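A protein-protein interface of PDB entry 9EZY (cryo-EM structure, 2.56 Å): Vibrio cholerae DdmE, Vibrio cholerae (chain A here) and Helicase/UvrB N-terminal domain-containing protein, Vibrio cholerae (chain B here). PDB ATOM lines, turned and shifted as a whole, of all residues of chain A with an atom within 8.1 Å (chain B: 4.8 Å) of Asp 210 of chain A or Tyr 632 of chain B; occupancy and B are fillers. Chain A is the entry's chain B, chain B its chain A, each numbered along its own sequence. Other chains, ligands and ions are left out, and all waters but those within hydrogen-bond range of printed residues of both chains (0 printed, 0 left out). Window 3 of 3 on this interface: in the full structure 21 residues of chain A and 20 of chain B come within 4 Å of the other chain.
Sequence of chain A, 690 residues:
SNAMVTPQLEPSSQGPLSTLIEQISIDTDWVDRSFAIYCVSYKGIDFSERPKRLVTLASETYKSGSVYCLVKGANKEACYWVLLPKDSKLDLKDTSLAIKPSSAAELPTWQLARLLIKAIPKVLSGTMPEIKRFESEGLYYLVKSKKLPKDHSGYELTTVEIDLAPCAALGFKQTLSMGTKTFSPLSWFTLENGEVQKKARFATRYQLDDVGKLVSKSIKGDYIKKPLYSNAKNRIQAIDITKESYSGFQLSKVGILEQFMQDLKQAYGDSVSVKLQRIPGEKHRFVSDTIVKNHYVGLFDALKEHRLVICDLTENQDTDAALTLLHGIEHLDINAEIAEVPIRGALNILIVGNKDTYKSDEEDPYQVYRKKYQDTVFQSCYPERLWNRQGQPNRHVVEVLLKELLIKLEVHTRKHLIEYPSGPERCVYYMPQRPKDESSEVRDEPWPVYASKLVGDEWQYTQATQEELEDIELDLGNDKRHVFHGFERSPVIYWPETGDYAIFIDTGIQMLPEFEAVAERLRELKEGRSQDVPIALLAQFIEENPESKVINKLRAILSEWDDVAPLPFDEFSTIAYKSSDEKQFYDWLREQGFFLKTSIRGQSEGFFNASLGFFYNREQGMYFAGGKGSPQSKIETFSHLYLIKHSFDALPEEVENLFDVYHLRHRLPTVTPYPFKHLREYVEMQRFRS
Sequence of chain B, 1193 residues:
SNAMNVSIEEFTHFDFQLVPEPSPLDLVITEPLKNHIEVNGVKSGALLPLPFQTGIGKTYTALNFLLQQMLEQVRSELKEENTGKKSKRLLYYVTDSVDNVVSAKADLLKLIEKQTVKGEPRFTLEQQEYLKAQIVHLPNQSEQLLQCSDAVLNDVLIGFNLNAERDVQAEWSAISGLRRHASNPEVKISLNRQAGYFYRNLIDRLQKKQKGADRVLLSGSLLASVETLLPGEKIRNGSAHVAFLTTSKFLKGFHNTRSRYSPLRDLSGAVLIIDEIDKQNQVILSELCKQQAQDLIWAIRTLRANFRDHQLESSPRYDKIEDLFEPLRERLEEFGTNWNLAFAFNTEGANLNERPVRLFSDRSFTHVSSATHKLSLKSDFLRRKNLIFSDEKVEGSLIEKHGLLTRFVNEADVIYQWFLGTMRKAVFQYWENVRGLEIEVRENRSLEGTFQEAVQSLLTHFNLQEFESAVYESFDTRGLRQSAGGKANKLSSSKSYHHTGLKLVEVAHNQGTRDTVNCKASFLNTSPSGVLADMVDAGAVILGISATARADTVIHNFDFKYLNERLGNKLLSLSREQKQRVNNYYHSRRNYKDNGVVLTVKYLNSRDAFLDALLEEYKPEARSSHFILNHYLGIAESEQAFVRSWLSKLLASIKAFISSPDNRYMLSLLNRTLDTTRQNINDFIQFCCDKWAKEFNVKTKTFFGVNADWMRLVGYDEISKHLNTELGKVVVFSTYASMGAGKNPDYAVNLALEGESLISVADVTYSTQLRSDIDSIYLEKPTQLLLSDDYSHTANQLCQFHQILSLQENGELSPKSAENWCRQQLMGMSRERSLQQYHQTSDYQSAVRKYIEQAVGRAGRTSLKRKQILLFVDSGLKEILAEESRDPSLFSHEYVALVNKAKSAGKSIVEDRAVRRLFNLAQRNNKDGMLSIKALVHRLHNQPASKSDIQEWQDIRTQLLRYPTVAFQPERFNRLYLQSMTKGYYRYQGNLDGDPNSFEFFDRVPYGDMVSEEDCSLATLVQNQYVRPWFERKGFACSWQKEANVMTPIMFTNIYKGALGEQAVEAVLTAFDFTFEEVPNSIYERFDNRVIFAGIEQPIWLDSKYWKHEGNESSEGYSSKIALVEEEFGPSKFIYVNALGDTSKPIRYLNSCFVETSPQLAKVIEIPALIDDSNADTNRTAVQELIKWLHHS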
ATOM      1  N   LEU A 142     -14.770  -6.117 -26.105  1.00  0.00           N
ATOM      2  CA  LEU A 142     -14.713  -5.474 -24.801  1.00  0.00           C
ATOM      3  C   LEU A 142     -13.262  -5.305 -24.377  1.00  0.00           C
ATOM      4  O   LEU A 142     -12.472  -6.253 -24.436  1.00  0.00           O
ATOM      5  CB  LEU A 142     -15.479  -6.293 -23.766  1.00  0.00           C
ATOM      6  CG  LEU A 142     -15.555  -5.670 -22.371  1.00  0.00           C
ATOM      7  CD1 LEU A 142     -16.290  -4.346 -22.419  1.00  0.00           C
ATOM      8  CD2 LEU A 142     -16.229  -6.614 -21.396  1.00  0.00           C
ATOM      9  N   SER A 145     -14.118  -1.862 -18.592  1.00  0.00           N
ATOM     10  CA  SER A 145     -15.433  -1.676 -17.998  1.00  0.00           C
ATOM     11  C   SER A 145     -15.309  -0.820 -16.748  1.00  0.00           C
ATOM     12  O   SER A 145     -14.269  -0.805 -16.086  1.00  0.00           O
ATOM     13  CB  SER A 145     -16.086  -3.019 -17.646  1.00  0.00           C
ATOM     14  OG  SER A 145     -15.343  -3.703 -16.655  1.00  0.00           O
ATOM     15  N   TYR A 155     -22.268  -2.378 -15.638  1.00  0.00           N
ATOM     16  CA  TYR A 155     -21.006  -1.760 -16.011  1.00  0.00           C
ATOM     17  C   TYR A 155     -21.206  -0.848 -17.210  1.00  0.00           C
ATOM     18  O   TYR A 155     -22.086  -1.075 -18.045  1.00  0.00           O
ATOM     19  CB  TYR A 155     -19.943  -2.807 -16.367  1.00  0.00           C
ATOM     20  CG  TYR A 155     -19.816  -3.939 -15.378  1.00  0.00           C
ATOM     21  CD1 TYR A 155     -19.142  -3.765 -14.177  1.00  0.00           C
ATOM     22  CD2 TYR A 155     -20.356  -5.187 -15.651  1.00  0.00           C
ATOM     23  CE1 TYR A 155     -19.019  -4.801 -13.273  1.00  0.00           C
ATOM     24  CE2 TYR A 155     -20.237  -6.227 -14.754  1.00  0.00           C
ATOM     25  CZ  TYR A 155     -19.569  -6.030 -13.567  1.00  0.00           C
ATOM     26  OH  TYR A 155     -19.448  -7.065 -12.669  1.00  0.00           O
ATOM     27  N   GLN A 207     -26.086  -6.812 -25.856  1.00  0.00           N
ATOM     28  CA  GLN A 207     -25.794  -7.783 -24.761  1.00  0.00           C
ATOM     29  C   GLN A 207     -24.301  -8.133 -24.727  1.00  0.00           C
ATOM     30  O   GLN A 207     -23.698  -8.231 -25.808  1.00  0.00           O
ATOM     31  CB  GLN A 207     -26.638  -9.048 -24.936  1.00  0.00           C
ATOM     32  CG  GLN A 207     -26.384 -10.119 -23.882  1.00  0.00           C
ATOM     33  CD  GLN A 207     -26.996  -9.786 -22.543  1.00  0.00           C
ATOM     34  OE1 GLN A 207     -26.418  -9.060 -21.737  1.00  0.00           O
ATOM     35  NE2 GLN A 207     -28.176 -10.327 -22.293  1.00  0.00           N
ATOM     36  N   LEU A 208     -23.730  -8.311 -23.531  1.00  0.00           N
ATOM     37  CA  LEU A 208     -22.294  -8.684 -23.406  1.00  0.00           C
ATOM     38  C   LEU A 208     -22.165 -10.207 -23.279  1.00  0.00           C
ATOM     39  O   LEU A 208     -23.095 -10.834 -22.734  1.00  0.00           O
ATOM     40  CB  LEU A 208     -21.683  -7.933 -22.218  1.00  0.00           C
ATOM     41  CG  LEU A 208     -21.255  -8.775 -21.017  1.00  0.00           C
ATOM     42  CD1 LEU A 208     -19.819  -8.460 -20.625  1.00  0.00           C
ATOM     43  CD2 LEU A 208     -22.189  -8.550 -19.838  1.00  0.00           C
ATOM     44  N   ASP A 209     -21.071 -10.779 -23.794  1.00  0.00           N
ATOM     45  CA  ASP A 209     -20.854 -12.251 -23.747  1.00  0.00           C
ATOM     46  C   ASP A 209     -20.531 -12.685 -22.313  1.00  0.00           C
ATOM     47  O   ASP A 209     -20.004 -11.852 -21.552  1.00  0.00           O
ATOM     48  CB  ASP A 209     -19.744 -12.671 -24.714  1.00  0.00           C
ATOM     49  CG  ASP A 209     -19.711 -14.158 -25.013  1.00  0.00           C
ATOM     50  OD1 ASP A 209     -20.748 -14.822 -24.808  1.00  0.00           O
ATOM     51  OD2 ASP A 209     -18.649 -14.643 -25.448  1.00  0.00           O
ATOM     52  N   ASP A 210     -20.824 -13.941 -21.963  1.00  0.00           N
ATOM     53  CA  ASP A 210     -20.466 -14.462 -20.616  1.00  0.00           C
ATOM     54  C   ASP A 210     -18.942 -14.411 -20.479  1.00  0.00           C
ATOM     55  O   ASP A 210     -18.461 -14.018 -19.398  1.00  0.00           O
ATOM     56  CB  ASP A 210     -21.024 -15.874 -20.413  1.00  0.00           C
ATOM     57  CG  ASP A 210     -20.309 -16.670 -19.336  1.00  0.00           C
ATOM     58  OD1 ASP A 210     -20.538 -16.381 -18.144  1.00  0.00           O
ATOM     59  OD2 ASP A 210     -19.533 -17.577 -19.696  1.00  0.00           O
ATOM     60  N   VAL A 211     -18.215 -14.774 -21.541  1.00  0.00           N
ATOM     61  CA  VAL A 211     -16.724 -14.676 -21.534  1.00  0.00           C
ATOM     62  C   VAL A 211     -16.350 -13.197 -21.391  1.00  0.00           C
ATOM     63  O   VAL A 211     -15.372 -12.900 -20.678  1.00  0.00           O
ATOM     64  CB  VAL A 211     -16.128 -15.292 -22.814  1.00  0.00           C
ATOM     65  CG1 VAL A 211     -14.611 -15.184 -22.855  1.00  0.00           C
ATOM     66  CG2 VAL A 211     -16.565 -16.737 -22.997  1.00  0.00           C
ATOM     67  N   GLY A 212     -17.114 -12.307 -22.032  1.00  0.00           N
ATOM     68  CA  GLY A 212     -16.808 -10.863 -21.996  1.00  0.00           C
ATOM     69  C   GLY A 212     -15.893 -10.470 -23.140  1.00  0.00           C
ATOM     70  O   GLY A 212     -15.495  -9.301 -23.197  1.00  0.00           O
ATOM     71  N   LYS A 213     -15.541 -11.425 -24.000  1.00  0.00           N
ATOM     72  CA  LYS A 213     -14.709 -11.121 -25.194  1.00  0.00           C
ATOM     73  C   LYS A 213     -15.476 -10.225 -26.174  1.00  0.00           C
ATOM     74  O   LYS A 213     -14.846  -9.308 -26.737  1.00  0.00           O
ATOM     75  CB  LYS A 213     -14.264 -12.426 -25.866  1.00  0.00           C
ATOM     76  CG  LYS A 213     -13.340 -12.273 -27.067  1.00  0.00           C
ATOM     77  CD  LYS A 213     -12.899 -13.596 -27.655  1.00  0.00           C
ATOM     78  CE  LYS A 213     -12.002 -13.432 -28.863  1.00  0.00           C
ATOM     79  NZ  LYS A 213     -11.585 -14.741 -29.418  1.00  0.00           N
ATOM     80  N   LEU A 214     -16.783 -10.451 -26.350  1.00  0.00           N
ATOM     81  CA  LEU A 214     -17.521  -9.716 -27.415  1.00  0.00           C
ATOM     82  C   LEU A 214     -18.835  -9.098 -26.924  1.00  0.00           C
ATOM     83  O   LEU A 214     -19.373  -9.588 -25.916  1.00  0.00           O
ATOM     84  CB  LEU A 214     -17.811 -10.730 -28.525  1.00  0.00           C
ATOM     85  CG  LEU A 214     -17.409 -10.306 -29.933  1.00  0.00           C
ATOM     86  CD1 LEU A 214     -16.930 -11.508 -30.733  1.00  0.00           C
ATOM     87  CD2 LEU A 214     -18.575  -9.627 -30.629  1.00  0.00           C
ATOM     88  N   LYS B 619     -10.650 -17.588 -13.796  1.00  0.00           N
ATOM     89  CA  LYS B 619     -11.228 -17.323 -15.108  1.00  0.00           C
ATOM     90  C   LYS B 619     -10.221 -17.738 -16.173  1.00  0.00           C
ATOM     91  O   LYS B 619      -9.701 -16.888 -16.905  1.00  0.00           O
ATOM     92  CB  LYS B 619     -11.604 -15.848 -15.272  1.00  0.00           C
ATOM     93  CG  LYS B 619     -12.482 -15.298 -14.167  1.00  0.00           C
ATOM     94  CD  LYS B 619     -13.854 -15.947 -14.194  1.00  0.00           C
ATOM     95  CE  LYS B 619     -14.829 -15.234 -13.279  1.00  0.00           C
ATOM     96  NZ  LYS B 619     -14.661 -15.655 -11.868  1.00  0.00           N
ATOM     97  N   PHE B 627      -7.433  -7.170 -18.020  1.00  0.00           N
ATOM     98  CA  PHE B 627      -8.883  -7.212 -18.160  1.00  0.00           C
ATOM     99  C   PHE B 627      -9.528  -7.961 -17.001  1.00  0.00           C
ATOM    100  O   PHE B 627     -10.563  -7.533 -16.477  1.00  0.00           O
ATOM    101  CB  PHE B 627      -9.262  -7.865 -19.487  1.00  0.00           C
ATOM    102  CG  PHE B 627     -10.739  -8.026 -19.678  1.00  0.00           C
ATOM    103  CD1 PHE B 627     -11.559  -6.921 -19.801  1.00  0.00           C
ATOM    104  CD2 PHE B 627     -11.309  -9.285 -19.727  1.00  0.00           C
ATOM    105  CE1 PHE B 627     -12.918  -7.067 -19.973  1.00  0.00           C
ATOM    106  CE2 PHE B 627     -12.667  -9.437 -19.898  1.00  0.00           C
ATOM    107  CZ  PHE B 627     -13.472  -8.328 -20.020  1.00  0.00           C
ATOM    108  N   ILE B 628      -8.931  -9.079 -16.587  1.00  0.00           N
ATOM    109  CA  ILE B 628      -9.498  -9.858 -15.489  1.00  0.00           C
ATOM    110  C   ILE B 628      -9.538  -9.020 -14.219  1.00  0.00           C
ATOM    111  O   ILE B 628     -10.539  -9.002 -13.494  1.00  0.00           O
ATOM    112  CB  ILE B 628      -8.696 -11.155 -15.283  1.00  0.00           C
ATOM    113  CG1 ILE B 628      -8.852 -12.076 -16.494  1.00  0.00           C
ATOM    114  CG2 ILE B 628      -9.155 -11.869 -14.024  1.00  0.00           C
ATOM    115  CD1 ILE B 628      -7.721 -13.063 -16.655  1.00  0.00           C
ATOM    116  N   LEU B 629      -8.446  -8.310 -13.930  1.00  0.00           N
ATOM    117  CA  LEU B 629      -8.420  -7.448 -12.756  1.00  0.00           C
ATOM    118  C   LEU B 629      -9.439  -6.324 -12.878  1.00  0.00           C
ATOM    119  O   LEU B 629     -10.128  -5.989 -11.907  1.00  0.00           O
ATOM    120  CB  LEU B 629      -7.015  -6.876 -12.561  1.00  0.00           C
ATOM    121  CG  LEU B 629      -6.786  -6.080 -11.275  1.00  0.00           C
ATOM    122  CD1 LEU B 629      -6.302  -6.987 -10.162  1.00  0.00           C
ATOM    123  CD2 LEU B 629      -5.798  -4.959 -11.515  1.00  0.00           C
ATOM    124  N   ASN B 630      -9.547  -5.723 -14.064  1.00  0.00           N
ATOM    125  CA  ASN B 630     -10.453  -4.593 -14.242  1.00  0.00           C
ATOM    126  C   ASN B 630     -11.909  -5.040 -14.263  1.00  0.00           C
ATOM    127  O   ASN B 630     -12.767  -4.425 -13.622  1.00  0.00           O
ATOM    128  CB  ASN B 630     -10.106  -3.850 -15.530  1.00  0.00           C
ATOM    129  CG  ASN B 630     -11.200  -2.900 -15.965  1.00  0.00           C
ATOM    130  OD1 ASN B 630     -11.665  -2.953 -17.102  1.00  0.00           O
ATOM    131  ND2 ASN B 630     -11.621  -2.027 -15.060  1.00  0.00           N
ATOM    132  N   HIS B 631     -12.210  -6.110 -14.998  1.00  0.00           N
ATOM    133  CA  HIS B 631     -13.603  -6.476 -15.230  1.00  0.00           C
ATOM    134  C   HIS B 631     -14.155  -7.341 -14.105  1.00  0.00           C
ATOM    135  O   HIS B 631     -15.230  -7.054 -13.564  1.00  0.00           O
ATOM    136  CB  HIS B 631     -13.734  -7.201 -16.570  1.00  0.00           C
ATOM    137  CG  HIS B 631     -15.148  -7.511 -16.950  1.00  0.00           C
ATOM    138  ND1 HIS B 631     -16.136  -6.552 -16.989  1.00  0.00           N
ATOM    139  CD2 HIS B 631     -15.740  -8.675 -17.311  1.00  0.00           C
ATOM    140  CE1 HIS B 631     -17.276  -7.111 -17.354  1.00  0.00           C
ATOM    141  NE2 HIS B 631     -17.062  -8.397 -17.556  1.00  0.00           N
ATOM    142  N   TYR B 632     -13.440  -8.401 -13.738  1.00  0.00           N
ATOM    143  CA  TYR B 632     -13.964  -9.364 -12.777  1.00  0.00           C
ATOM    144  C   TYR B 632     -13.686  -8.955 -11.338  1.00  0.00           C
ATOM    145  O   TYR B 632     -14.559  -9.101 -10.475  1.00  0.00           O
ATOM    146  CB  TYR B 632     -13.376 -10.746 -13.057  1.00  0.00           C
ATOM    147  CG  TYR B 632     -13.912 -11.363 -14.325  1.00  0.00           C
ATOM    148  CD1 TYR B 632     -15.229 -11.794 -14.407  1.00  0.00           C
ATOM    149  CD2 TYR B 632     -13.108 -11.507 -15.445  1.00  0.00           C
ATOM    150  CE1 TYR B 632     -15.725 -12.354 -15.564  1.00  0.00           C
ATOM    151  CE2 TYR B 632     -13.596 -12.066 -16.606  1.00  0.00           C
ATOM    152  CZ  TYR B 632     -14.905 -12.488 -16.661  1.00  0.00           C
ATOM    153  OH  TYR B 632     -15.394 -13.047 -17.817  1.00  0.00           O
ATOM    154  N   LEU B 633     -12.489  -8.445 -11.054  1.00  0.00           N
ATOM    155  CA  LEU B 633     -12.196  -7.918  -9.730  1.00  0.00           C
ATOM    156  C   LEU B 633     -12.701  -6.494  -9.545  1.00  0.00           C
ATOM    157  O   LEU B 633     -12.631  -5.970  -8.428  1.00  0.00           O
ATOM    158  CB  LEU B 633     -10.691  -7.977  -9.460  1.00  0.00           C
ATOM    159  CG  LEU B 633     -10.187  -9.339  -8.979  1.00  0.00           C
ATOM    160  CD1 LEU B 633     -10.264 -10.367 -10.094  1.00  0.00           C
ATOM    161  CD2 LEU B 633      -8.768  -9.241  -8.448  1.00  0.00           C
ATOM    162  N   GLY B 634     -13.204  -5.860 -10.602  1.00  0.00           N
ATOM    163  CA  GLY B 634     -13.820  -4.556 -10.478  1.00  0.00           C
ATOM    164  C   GLY B 634     -12.902  -3.450 -10.019  1.00  0.00           C
ATOM    165  O   GLY B 634     -13.294  -2.658  -9.158  1.00  0.00           O
ATOM    166  N   ASN B 680     -15.476  -8.986  -4.711  1.00  0.00           N
ATOM    167  CA  ASN B 680     -14.851  -9.451  -5.944  1.00  0.00           C
ATOM    168  C   ASN B 680     -13.397  -9.841  -5.719  1.00  0.00           C
ATOM    169  O   ASN B 680     -12.920 -10.817  -6.306  1.00  0.00           O
ATOM    170  CB  ASN B 680     -14.957  -8.371  -7.018  1.00  0.00           C
ATOM    171  CG  ASN B 680     -16.391  -8.081  -7.409  1.00  0.00           C
ATOM    172  OD1 ASN B 680     -17.208  -8.992  -7.532  1.00  0.00           O
ATOM    173  ND2 ASN B 680     -16.706  -6.806  -7.598  1.00  0.00           N
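The backbone carbonyl oxygen (O) of Lys 213 of chain A sits at hydrogen-bond distance from the backbone NH (N) of Leu 142 of chain A, 3.3 Å away.
Among the printed residues, pairs that only touch across the chains: Leu 142 of chain A with Phe 627 of chain B (3.5 Å), Asp 210 of chain A with Tyr 632 of chain B (3.6 Å) and Gly 212 of chain A with Phe 627 of chain B (3.9 Å).
The side-chain hydroxyl (OH) of Tyr 632 of chain B sits at hydrogen-bond distance from the backbone carbonyl oxygen (O) of Val 211 of chain A, 2.9 Å away. The side-chain amide oxygen (OD1) of Asn 630 of chain B is in hydrogen-bond range of the backbone NH (N) of Ser 145 of chain A, at 3.1 Å. The side-chain hydroxyl of Ser 145 of chain A is in hydrogen-bond range of a ring nitrogen (ND1) of His 631 of chain B (3.0 Å).
Asp 210 of chain A touches one residue of chain B. Printed residues of chain A within 4 Å of Tyr 632 of chain B: Asp 210 (3.6 Å) and Val 211 (2.9 Å). Of the printed residues of chain B, Gly 212 of chain A touches Phe 627. Of the printed residues of chain B, Leu 142 of chain A touches Phe 627 (3.5 Å). Printed residues of chain A within 4 Å of Phe 627 of chain B: Leu 142 (3.5 Å) and Gly 212 (3.9 Å). Of the printed residues of chain B, Val 211 of chain A touches Tyr 632 (2.9 Å). Of the printed residues of chain B, Ser 145 of chain A touches Asn 630 (3.1 Å) and His 631 (3.0 Å). Gln 207 of chain A touches none of the printed residues of chain B. The nearest residue of chain A that does not touch Tyr 632 of chain B is Gly 212 of chain A (4.6 Å).
Of the 11 printed residues of chain A, 5 touch a printed residue of chain B. Of the 10 printed residues of chain B, 4 touch a printed residue of chain A. Hydrophobic or aromatic side chains of chain B that line the printed part of chain A: Phe 627, His 631 and Tyr 632. Among the printed residues, 6 pairs touch across the chains. Among the printed residues, no Asp or Glu carboxylate lies within 4 Å of a Lys or Arg side-chain nitrogen of the other chain.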
